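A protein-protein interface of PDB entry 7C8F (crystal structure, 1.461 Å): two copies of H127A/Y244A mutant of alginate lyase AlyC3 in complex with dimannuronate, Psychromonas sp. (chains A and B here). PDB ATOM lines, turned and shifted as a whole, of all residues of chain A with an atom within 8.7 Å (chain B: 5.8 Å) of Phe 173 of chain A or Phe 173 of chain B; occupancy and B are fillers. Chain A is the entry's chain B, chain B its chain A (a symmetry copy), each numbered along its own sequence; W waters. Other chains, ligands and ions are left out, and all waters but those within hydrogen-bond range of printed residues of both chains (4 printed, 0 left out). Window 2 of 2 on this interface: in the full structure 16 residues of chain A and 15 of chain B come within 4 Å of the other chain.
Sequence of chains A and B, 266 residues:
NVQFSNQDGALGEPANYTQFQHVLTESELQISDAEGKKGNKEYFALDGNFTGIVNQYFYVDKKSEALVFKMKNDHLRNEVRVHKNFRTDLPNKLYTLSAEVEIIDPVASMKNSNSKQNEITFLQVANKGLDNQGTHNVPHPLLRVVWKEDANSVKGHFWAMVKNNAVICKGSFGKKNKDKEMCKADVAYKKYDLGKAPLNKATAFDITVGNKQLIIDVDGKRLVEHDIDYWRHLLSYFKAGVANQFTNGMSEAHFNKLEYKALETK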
ATOM      1  N   THR A 135      -6.862  -7.096   7.169  1.00  0.00           N
ATOM      2  CA  THR A 135      -6.854  -7.119   8.625  1.00  0.00           C
ATOM      3  C   THR A 135      -6.574  -8.530   9.135  1.00  0.00           C
ATOM      4  O   THR A 135      -7.178  -9.509   8.678  1.00  0.00           O
ATOM      5  CB  THR A 135      -8.206  -6.626   9.135  1.00  0.00           C
ATOM      6  OG1 THR A 135      -8.502  -5.376   8.501  1.00  0.00           O
ATOM      7  CG2 THR A 135      -8.196  -6.437  10.637  1.00  0.00           C
ATOM      8  N   HIS A 136      -5.653  -8.637  10.089  1.00  0.00           N
ATOM      9  CA  HIS A 136      -5.308  -9.929  10.688  1.00  0.00           C
ATOM     10  C   HIS A 136      -4.864 -10.947   9.636  1.00  0.00           C
ATOM     11  O   HIS A 136      -5.205 -12.131   9.690  1.00  0.00           O
ATOM     12  CB  HIS A 136      -6.428 -10.460  11.595  1.00  0.00           C
ATOM     13  CG  HIS A 136      -6.598  -9.661  12.852  1.00  0.00           C
ATOM     14  ND1 HIS A 136      -5.564  -9.459  13.740  1.00  0.00           N
ATOM     15  CD2 HIS A 136      -7.673  -9.018  13.371  1.00  0.00           C
ATOM     16  CE1 HIS A 136      -5.994  -8.726  14.754  1.00  0.00           C
ATOM     17  NE2 HIS A 136      -7.269  -8.441  14.552  1.00  0.00           N
ATOM     18  N   ASN A 137      -4.086 -10.476   8.668  1.00  0.00           N
ATOM     19  CA  ASN A 137      -3.468 -11.370   7.694  1.00  0.00           C
ATOM     20  C   ASN A 137      -2.657 -12.451   8.395  1.00  0.00           C
ATOM     21  O   ASN A 137      -1.968 -12.193   9.385  1.00  0.00           O
ATOM     22  CB  ASN A 137      -2.533 -10.545   6.812  1.00  0.00           C
ATOM     23  CG  ASN A 137      -1.659 -11.403   5.925  1.00  0.00           C
ATOM     24  OD1 ASN A 137      -0.497 -11.686   6.249  1.00  0.00           O
ATOM     25  ND2 ASN A 137      -2.216 -11.844   4.806  1.00  0.00           N
ATOM     26  N   VAL A 138      -2.723 -13.669   7.871  1.00  0.00           N
ATOM     27  CA  VAL A 138      -1.891 -14.774   8.338  1.00  0.00           C
ATOM     28  C   VAL A 138      -0.733 -14.914   7.353  1.00  0.00           C
ATOM     29  O   VAL A 138      -0.980 -15.076   6.151  1.00  0.00           O
ATOM     30  CB  VAL A 138      -2.709 -16.070   8.445  1.00  0.00           C
ATOM     31  CG1 VAL A 138      -1.818 -17.269   8.769  1.00  0.00           C
ATOM     32  CG2 VAL A 138      -3.784 -15.894   9.518  1.00  0.00           C
ATOM     33  N   PRO A 139       0.533 -14.804   7.797  1.00  0.00           N
ATOM     34  CA  PRO A 139       1.646 -14.700   6.835  1.00  0.00           C
ATOM     35  C   PRO A 139       2.121 -16.046   6.308  1.00  0.00           C
ATOM     36  O   PRO A 139       3.329 -16.288   6.183  1.00  0.00           O
ATOM     37  CB  PRO A 139       2.740 -14.004   7.657  1.00  0.00           C
ATOM     38  CG  PRO A 139       2.519 -14.501   9.033  1.00  0.00           C
ATOM     39  CD  PRO A 139       0.991 -14.627   9.186  1.00  0.00           C
ATOM     40  N   HIS A 140       1.172 -16.930   5.998  1.00  0.00           N
ATOM     41  CA  HIS A 140       1.433 -18.264   5.490  1.00  0.00           C
ATOM     42  C   HIS A 140       0.376 -18.452   4.405  1.00  0.00           C
ATOM     43  O   HIS A 140      -0.817 -18.184   4.657  1.00  0.00           O
ATOM     44  CB  HIS A 140       1.237 -19.348   6.558  1.00  0.00           C
ATOM     45  CG  HIS A 140       1.964 -19.099   7.848  1.00  0.00           C
ATOM     46  ND1 HIS A 140       3.324 -19.282   7.985  1.00  0.00           N
ATOM     47  CD2 HIS A 140       1.513 -18.710   9.065  1.00  0.00           C
ATOM     48  CE1 HIS A 140       3.682 -19.005   9.229  1.00  0.00           C
ATOM     49  NE2 HIS A 140       2.602 -18.658   9.908  1.00  0.00           N
ATOM     50  N   VAL A 167      -3.051 -20.626  12.191  1.00  0.00           N
ATOM     51  CA  VAL A 167      -2.243 -20.048  13.258  1.00  0.00           C
ATOM     52  C   VAL A 167      -1.071 -19.280  12.671  1.00  0.00           C
ATOM     53  O   VAL A 167      -0.416 -19.739  11.723  1.00  0.00           O
ATOM     54  CB  VAL A 167      -1.754 -21.163  14.197  1.00  0.00           C
ATOM     55  CG1 VAL A 167      -0.867 -20.590  15.340  1.00  0.00           C
ATOM     56  CG2 VAL A 167      -2.933 -21.928  14.739  1.00  0.00           C
ATOM     57  N   ILE A 168      -0.788 -18.110  13.237  1.00  0.00           N
ATOM     58  CA  ILE A 168       0.404 -17.352  12.858  1.00  0.00           C
ATOM     59  C   ILE A 168       1.596 -17.935  13.604  1.00  0.00           C
ATOM     60  O   ILE A 168       1.625 -17.926  14.840  1.00  0.00           O
ATOM     61  CB  ILE A 168       0.239 -15.859  13.166  1.00  0.00           C
ATOM     62  CG1 ILE A 168      -0.935 -15.295  12.370  1.00  0.00           C
ATOM     63  CG2 ILE A 168       1.519 -15.104  12.803  1.00  0.00           C
ATOM     64  CD1 ILE A 168      -1.166 -13.822  12.604  1.00  0.00           C
ATOM     65  N   CYS A 169       2.582 -18.442  12.855  1.00  0.00           N
ATOM     66  CA  CYS A 169       3.680 -19.205  13.436  1.00  0.00           C
ATOM     67  C   CYS A 169       5.036 -18.533  13.291  1.00  0.00           C
ATOM     68  O   CYS A 169       6.044 -19.116  13.716  1.00  0.00           O
ATOM     69  CB  CYS A 169       3.741 -20.618  12.834  1.00  0.00           C
ATOM     70  SG  CYS A 169       2.383 -21.678  13.309  1.00  0.00           S
ATOM     71  N   LYS A 170       5.095 -17.349  12.691  1.00  0.00           N
ATOM     72  CA  LYS A 170       6.350 -16.631  12.531  1.00  0.00           C
ATOM     73  C   LYS A 170       6.057 -15.140  12.551  1.00  0.00           C
ATOM     74  O   LYS A 170       4.906 -14.708  12.464  1.00  0.00           O
ATOM     75  CB  LYS A 170       7.047 -17.014  11.225  1.00  0.00           C
ATOM     76  CG  LYS A 170       6.324 -16.522   9.988  1.00  0.00           C
ATOM     77  CD  LYS A 170       6.891 -17.140   8.701  1.00  0.00           C
ATOM     78  CE  LYS A 170       6.180 -16.578   7.479  1.00  0.00           C
ATOM     79  NZ  LYS A 170       6.657 -17.192   6.202  1.00  0.00           N
ATOM     80  N   GLY A 171       7.120 -14.350  12.654  1.00  0.00           N
ATOM     81  CA  GLY A 171       6.977 -12.913  12.632  1.00  0.00           C
ATOM     82  C   GLY A 171       6.512 -12.344  13.959  1.00  0.00           C
ATOM     83  O   GLY A 171       6.344 -13.037  14.965  1.00  0.00           O
ATOM     84  N   SER A 172       6.284 -11.029  13.940  1.00  0.00           N
ATOM     85  CA  SER A 172       5.972 -10.311  15.172  1.00  0.00           C
ATOM     86  C   SER A 172       4.728 -10.860  15.856  1.00  0.00           C
ATOM     87  O   SER A 172       4.644 -10.849  17.089  1.00  0.00           O
ATOM     88  CB  SER A 172       5.815  -8.818  14.883  1.00  0.00           C
ATOM     89  OG  SER A 172       4.820  -8.586  13.901  1.00  0.00           O
ATOM     90  N   PHE A 173       3.758 -11.344  15.086  1.00  0.00           N
ATOM     91  CA  PHE A 173       2.502 -11.826  15.641  1.00  0.00           C
ATOM     92  C   PHE A 173       2.495 -13.332  15.893  1.00  0.00           C
ATOM     93  O   PHE A 173       1.443 -13.887  16.224  1.00  0.00           O
ATOM     94  CB  PHE A 173       1.331 -11.416  14.741  1.00  0.00           C
ATOM     95  CG  PHE A 173       1.116  -9.926  14.671  1.00  0.00           C
ATOM     96  CD1 PHE A 173       0.517  -9.250  15.721  1.00  0.00           C
ATOM     97  CD2 PHE A 173       1.519  -9.204  13.560  1.00  0.00           C
ATOM     98  CE1 PHE A 173       0.322  -7.878  15.662  1.00  0.00           C
ATOM     99  CE2 PHE A 173       1.327  -7.834  13.493  1.00  0.00           C
ATOM    100  CZ  PHE A 173       0.727  -7.173  14.546  1.00  0.00           C
ATOM    101  N   GLY A 174       3.636 -14.001  15.756  1.00  0.00           N
ATOM    102  CA  GLY A 174       3.692 -15.430  15.980  1.00  0.00           C
ATOM    103  C   GLY A 174       4.526 -15.821  17.182  1.00  0.00           C
ATOM    104  O   GLY A 174       4.716 -17.010  17.451  1.00  0.00           O
ATOM    105  N   LYS A 175       5.013 -14.825  17.928  1.00  0.00           N
ATOM    106  CA  LYS A 175       5.939 -15.109  19.023  1.00  0.00           C
ATOM    107  C   LYS A 175       5.323 -16.047  20.054  1.00  0.00           C
ATOM    108  O   LYS A 175       6.006 -16.925  20.591  1.00  0.00           O
ATOM    109  CB  LYS A 175       6.406 -13.804  19.670  1.00  0.00           C
ATOM    110  CG  LYS A 175       7.505 -13.096  18.896  1.00  0.00           C
ATOM    111  CD  LYS A 175       7.498 -11.599  19.154  1.00  0.00           C
ATOM    112  CE  LYS A 175       8.685 -10.924  18.486  1.00  0.00           C
ATOM    113  NZ  LYS A 175       8.472  -9.462  18.323  1.00  0.00           N
ATOM    114  N   LYS A 176       4.029 -15.888  20.332  1.00  0.00           N
ATOM    115  CA  LYS A 176       3.374 -16.707  21.343  1.00  0.00           C
ATOM    116  C   LYS A 176       3.094 -18.125  20.857  1.00  0.00           C
ATOM    117  O   LYS A 176       2.877 -19.019  21.682  1.00  0.00           O
ATOM    118  CB  LYS A 176       2.074 -16.035  21.791  1.00  0.00           C
ATOM    119  CG  LYS A 176       1.298 -16.804  22.839  1.00  0.00           C
ATOM    120  CD  LYS A 176       0.121 -15.990  23.355  1.00  0.00           C
ATOM    121  CE  LYS A 176      -0.603 -16.733  24.468  1.00  0.00           C
ATOM    122  NZ  LYS A 176      -1.711 -15.930  25.062  1.00  0.00           N
ATOM    123  N   ASN A 177       3.105 -18.354  19.542  1.00  0.00           N
ATOM    124  CA  ASN A 177       2.744 -19.652  18.984  1.00  0.00           C
ATOM    125  C   ASN A 177       3.924 -20.449  18.447  1.00  0.00           C
ATOM    126  O   ASN A 177       3.821 -21.678  18.353  1.00  0.00           O
ATOM    127  CB  ASN A 177       1.749 -19.473  17.824  1.00  0.00           C
ATOM    128  CG  ASN A 177       0.527 -18.663  18.214  1.00  0.00           C
ATOM    129  OD1 ASN A 177      -0.006 -18.820  19.306  1.00  0.00           O
ATOM    130  ND2 ASN A 177       0.079 -17.801  17.316  1.00  0.00           N
ATOM    131  N   LYS A 178       5.028 -19.788  18.100  1.00  0.00           N
ATOM    132  CA  LYS A 178       6.033 -20.405  17.236  1.00  0.00           C
ATOM    133  C   LYS A 178       6.636 -21.671  17.836  1.00  0.00           C
ATOM    134  O   LYS A 178       7.063 -22.559  17.089  1.00  0.00           O
ATOM    135  CB  LYS A 178       7.129 -19.398  16.897  1.00  0.00           C
ATOM    136  CG  LYS A 178       8.033 -19.045  18.062  1.00  0.00           C
ATOM    137  CD  LYS A 178       9.179 -18.150  17.605  1.00  0.00           C
ATOM    138  CE  LYS A 178      10.167 -17.895  18.733  1.00  0.00           C
ATOM    139  NZ  LYS A 178       9.513 -17.220  19.888  1.00  0.00           N
ATOM    140  N   CYS A 183       2.628 -25.264  15.662  1.00  0.00           N
ATOM    141  CA  CYS A 183       3.507 -24.590  14.722  1.00  0.00           C
ATOM    142  C   CYS A 183       4.670 -25.451  14.243  1.00  0.00           C
ATOM    143  O   CYS A 183       5.492 -24.969  13.461  1.00  0.00           O
ATOM    144  CB  CYS A 183       4.020 -23.276  15.317  1.00  0.00           C
ATOM    145  SG  CYS A 183       2.739 -21.980  15.304  1.00  0.00           S
ATOM    146  N   HIS B 136      -4.940 -17.168  19.360  1.00  0.00           N
ATOM    147  CA  HIS B 136      -5.478 -15.990  18.678  1.00  0.00           C
ATOM    148  C   HIS B 136      -6.789 -15.505  19.304  1.00  0.00           C
ATOM    149  O   HIS B 136      -7.727 -15.097  18.613  1.00  0.00           O
ATOM    150  CB  HIS B 136      -5.589 -16.209  17.167  1.00  0.00           C
ATOM    151  CG  HIS B 136      -4.259 -16.281  16.481  1.00  0.00           C
ATOM    152  ND1 HIS B 136      -3.319 -15.281  16.592  1.00  0.00           N
ATOM    153  CD2 HIS B 136      -3.700 -17.239  15.704  1.00  0.00           C
ATOM    154  CE1 HIS B 136      -2.243 -15.611  15.898  1.00  0.00           C
ATOM    155  NE2 HIS B 136      -2.448 -16.793  15.345  1.00  0.00           N
ATOM    156  N   ILE B 168      -9.110  -7.266  16.584  1.00  0.00           N
ATOM    157  CA  ILE B 168      -8.494  -6.907  17.859  1.00  0.00           C
ATOM    158  C   ILE B 168      -8.221  -5.411  17.839  1.00  0.00           C
ATOM    159  O   ILE B 168      -7.443  -4.926  17.011  1.00  0.00           O
ATOM    160  CB  ILE B 168      -7.209  -7.700  18.107  1.00  0.00           C
ATOM    161  CG1 ILE B 168      -7.525  -9.193  18.101  1.00  0.00           C
ATOM    162  CG2 ILE B 168      -6.578  -7.286  19.439  1.00  0.00           C
ATOM    163  CD1 ILE B 168      -6.324 -10.075  18.378  1.00  0.00           C
ATOM    164  N   LYS B 170      -7.520  -3.463  20.803  1.00  0.00           N
ATOM    165  CA  LYS B 170      -6.785  -2.959  21.953  1.00  0.00           C
ATOM    166  C   LYS B 170      -5.713  -3.963  22.344  1.00  0.00           C
ATOM    167  O   LYS B 170      -5.700  -5.107  21.881  1.00  0.00           O
ATOM    168  CB  LYS B 170      -7.716  -2.692  23.138  1.00  0.00           C
ATOM    169  CG  LYS B 170      -8.285  -3.948  23.756  1.00  0.00           C
ATOM    170  CD  LYS B 170      -9.358  -3.604  24.794  1.00  0.00           C
ATOM    171  CE  LYS B 170      -9.907  -4.842  25.465  1.00  0.00           C
ATOM    172  NZ  LYS B 170     -11.036  -4.473  26.369  1.00  0.00           N
ATOM    173  N   GLY B 171      -4.813  -3.525  23.221  1.00  0.00           N
ATOM    174  CA  GLY B 171      -3.758  -4.387  23.707  1.00  0.00           C
ATOM    175  C   GLY B 171      -2.619  -4.544  22.715  1.00  0.00           C
ATOM    176  O   GLY B 171      -2.581  -3.939  21.648  1.00  0.00           O
ATOM    177  N   SER B 172      -1.669  -5.405  23.090  1.00  0.00           N
ATOM    178  CA  SER B 172      -0.446  -5.538  22.304  1.00  0.00           C
ATOM    179  C   SER B 172      -0.725  -5.985  20.874  1.00  0.00           C
ATOM    180  O   SER B 172       0.028  -5.635  19.959  1.00  0.00           O
ATOM    181  CB  SER B 172       0.535  -6.491  22.992  1.00  0.00           C
ATOM    182  OG  SER B 172      -0.041  -7.767  23.195  1.00  0.00           O
ATOM    183  N   PHE B 173      -1.794  -6.748  20.652  1.00  0.00           N
ATOM    184  CA  PHE B 173      -2.115  -7.210  19.306  1.00  0.00           C
ATOM    185  C   PHE B 173      -3.103  -6.306  18.573  1.00  0.00           C
ATOM    186  O   PHE B 173      -3.532  -6.645  17.465  1.00  0.00           O
ATOM    187  CB  PHE B 173      -2.608  -8.661  19.337  1.00  0.00           C
ATOM    188  CG  PHE B 173      -1.581  -9.640  19.835  1.00  0.00           C
ATOM    189  CD1 PHE B 173      -0.557 -10.068  19.011  1.00  0.00           C
ATOM    190  CD2 PHE B 173      -1.635 -10.121  21.134  1.00  0.00           C
ATOM    191  CE1 PHE B 173       0.396 -10.964  19.468  1.00  0.00           C
ATOM    192  CE2 PHE B 173      -0.688 -11.018  21.600  1.00  0.00           C
ATOM    193  CZ  PHE B 173       0.330 -11.441  20.761  1.00  0.00           C
ATOM    194  N   GLY B 174      -3.467  -5.162  19.148  1.00  0.00           N
ATOM    195  CA  GLY B 174      -4.401  -4.277  18.484  1.00  0.00           C
ATOM    196  C   GLY B 174      -3.785  -2.993  17.972  1.00  0.00           C
ATOM    197  O   GLY B 174      -4.494  -2.120  17.467  1.00  0.00           O
ATOM    198  N   LYS B 175      -2.462  -2.859  18.078  1.00  0.00           N
ATOM    199  CA  LYS B 175      -1.841  -1.569  17.790  1.00  0.00           C
ATOM    200  C   LYS B 175      -2.045  -1.154  16.338  1.00  0.00           C
ATOM    201  O   LYS B 175      -2.229   0.033  16.043  1.00  0.00           O
ATOM    202  CB  LYS B 175      -0.359  -1.586  18.169  1.00  0.00           C
ATOM    203  CG  LYS B 175      -0.095  -1.180  19.614  1.00  0.00           C
ATOM    204  CD  LYS B 175       1.375  -0.839  19.839  1.00  0.00           C
ATOM    205  CE  LYS B 175       2.141  -2.007  20.444  1.00  0.00           C
ATOM    206  NZ  LYS B 175       1.712  -2.281  21.846  1.00  0.00           N
ATOM    207  N   LYS B 176      -2.031  -2.117  15.412  1.00  0.00           N
ATOM    208  CA  LYS B 176      -2.193  -1.793  14.001  1.00  0.00           C
ATOM    209  C   LYS B 176      -3.631  -1.455  13.632  1.00  0.00           C
ATOM    210  O   LYS B 176      -3.868  -0.886  12.562  1.00  0.00           O
ATOM    211  CB  LYS B 176      -1.707  -2.960  13.140  1.00  0.00           C
ATOM    212  CG  LYS B 176      -1.724  -2.684  11.656  1.00  0.00           C
ATOM    213  CD  LYS B 176      -1.208  -3.873  10.866  1.00  0.00           C
ATOM    214  CE  LYS B 176      -1.017  -3.489   9.410  1.00  0.00           C
ATOM    215  NZ  LYS B 176      -2.125  -2.605   8.944  1.00  0.00           N
ATOM    216  N   ASN B 177      -4.597  -1.798  14.485  1.00  0.00           N
ATOM    217  CA  ASN B 177      -6.001  -1.588  14.175  1.00  0.00           C
ATOM    218  C   ASN B 177      -6.657  -0.496  15.005  1.00  0.00           C
ATOM    219  O   ASN B 177      -7.693   0.028  14.582  1.00  0.00           O
ATOM    220  CB  ASN B 177      -6.794  -2.881  14.425  1.00  0.00           C
ATOM    221  CG  ASN B 177      -6.228  -4.077  13.687  1.00  0.00           C
ATOM    222  OD1 ASN B 177      -5.809  -3.972  12.527  1.00  0.00           O
ATOM    223  ND2 ASN B 177      -6.236  -5.230  14.349  1.00  0.00           N
HETATM  224  O   HOH W   1      -2.065 -16.996  20.027  1.00  0.00           O
HETATM  225  O   HOH W   2      -0.812 -13.101  17.225  1.00  0.00           O
HETATM  226  O   HOH W   3      -4.560  -6.221  11.436  1.00  0.00           O
HETATM  227  O   HOH W   4      -2.880  -8.501  15.604  1.00  0.00           O
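O of Ile 168 of chain A is in hydrogen-bond range of ND2 of Asn 177 of chain A (2.9 Å).
The side-chain amide nitrogen (ND2) of Asn 177 of chain B is in hydrogen-bond range of the backbone carbonyl oxygen (O) of Ile 168 of chain B.
The side-chain sulfur (SG) of Cys 169 of chain A is disulfide-bonded to the side-chain sulfur (SG) of Cys 183 of chain A (2.0 Å).
Water W2 lies within hydrogen-bond range of the backbone carbonyl oxygen (O) of Phe 173 of chain A and a ring nitrogen (ND1) of His 136 of chain B.
Water W4 bridges O of Phe 173 of chain B (2.7 Å) and ND1 of His 136 of chain A (3.4 Å).
Water W3 lies within hydrogen-bond range of the side-chain amide oxygen of Asn 177 of chain B and the backbone NH of His 136 of chain A.
Water W1 bridges OD1 of Asn 177 of chain A (2.8 Å) and N of His 136 of chain B (3.0 Å).
His 136 of chain A touches Ile 168 of chain B, and with the chains exchanged Ile 168 of chain A touches His 136 of chain B.
His 136 of chain A touches Asn 177 of chain B, and with the chains exchanged Asn 177 of chain A touches His 136 of chain B.
Phe 173 of chain A touches its own counterpart, Phe 173 of chain B.
Positions printed for both chains: 136, 168, 170, 171, 172, 173, 174, 175, 176 and 177.
Of the 7 pairs that touch across the chains among the printed residues, 5 have their exchanged pair printed and touching as well.
Phe 173 of chain A touches one residue of chain B.
Phe 173 of chain B touches just one residue of chain A: Phe 173 (3.6 Å).
No residue of chain A comes within 4 Å of Ser 172 of chain B.
No residue of chain A comes within 4 Å of Gly 174 of chain B.
Of the printed residues of chain B, Val 167 of chain A touches His 136.
Of the printed residues of chain B, Ile 168 of chain A touches His 136 (3.0 Å).
Printed residues of chain A within 4 Å of Asn 177 of chain B: Thr 135 and His 136.
Of the printed residues of chain A, Ile 168 of chain B touches His 136 (3.0 Å).
Lys 170 of chain B touches none of the printed residues of chain A.
The nearest printed residue of chain A that does not touch Asn 177 of chain B is Phe 173 of chain A (7.2 Å).
Among the printed residues, merely in contact across the chains: Thr 135 of chain A with Asn 177 of chain B (3.9 Å), Val 167 of chain A with His 136 of chain B (3.9 Å) and Phe 173 of chain A with Phe 173 of chain B (3.6 Å).
A ring nitrogen (NE2) of His 136 of chain A sits at hydrogen-bond distance from the backbone NH (N) of Ile 168 of chain B.
NE2 of His 136 of chain A is in hydrogen-bond range of ND2 of Asn 177 of chain B (3.4 Å).
NE2 of His 136 of chain B lies within hydrogen-bond range of N of Ile 168 of chain A (3.0 Å).
ND2 of Asn 177 of chain A sits at hydrogen-bond distance from NE2 of His 136 of chain B.
Hydrophobic or aromatic side chains of chain A within 4 Å of the printed part of chain B: His 136, Ile 168 and Phe 173.
Of the 10 printed residues of chain B, 4 touch a printed residue of chain A.
Hydrophobic or aromatic side chains of chain B within 4 Å of the printed part of chain A: His 136, Ile 168 and Phe 173.
Among the printed residues, 7 pairs touch across the chains.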
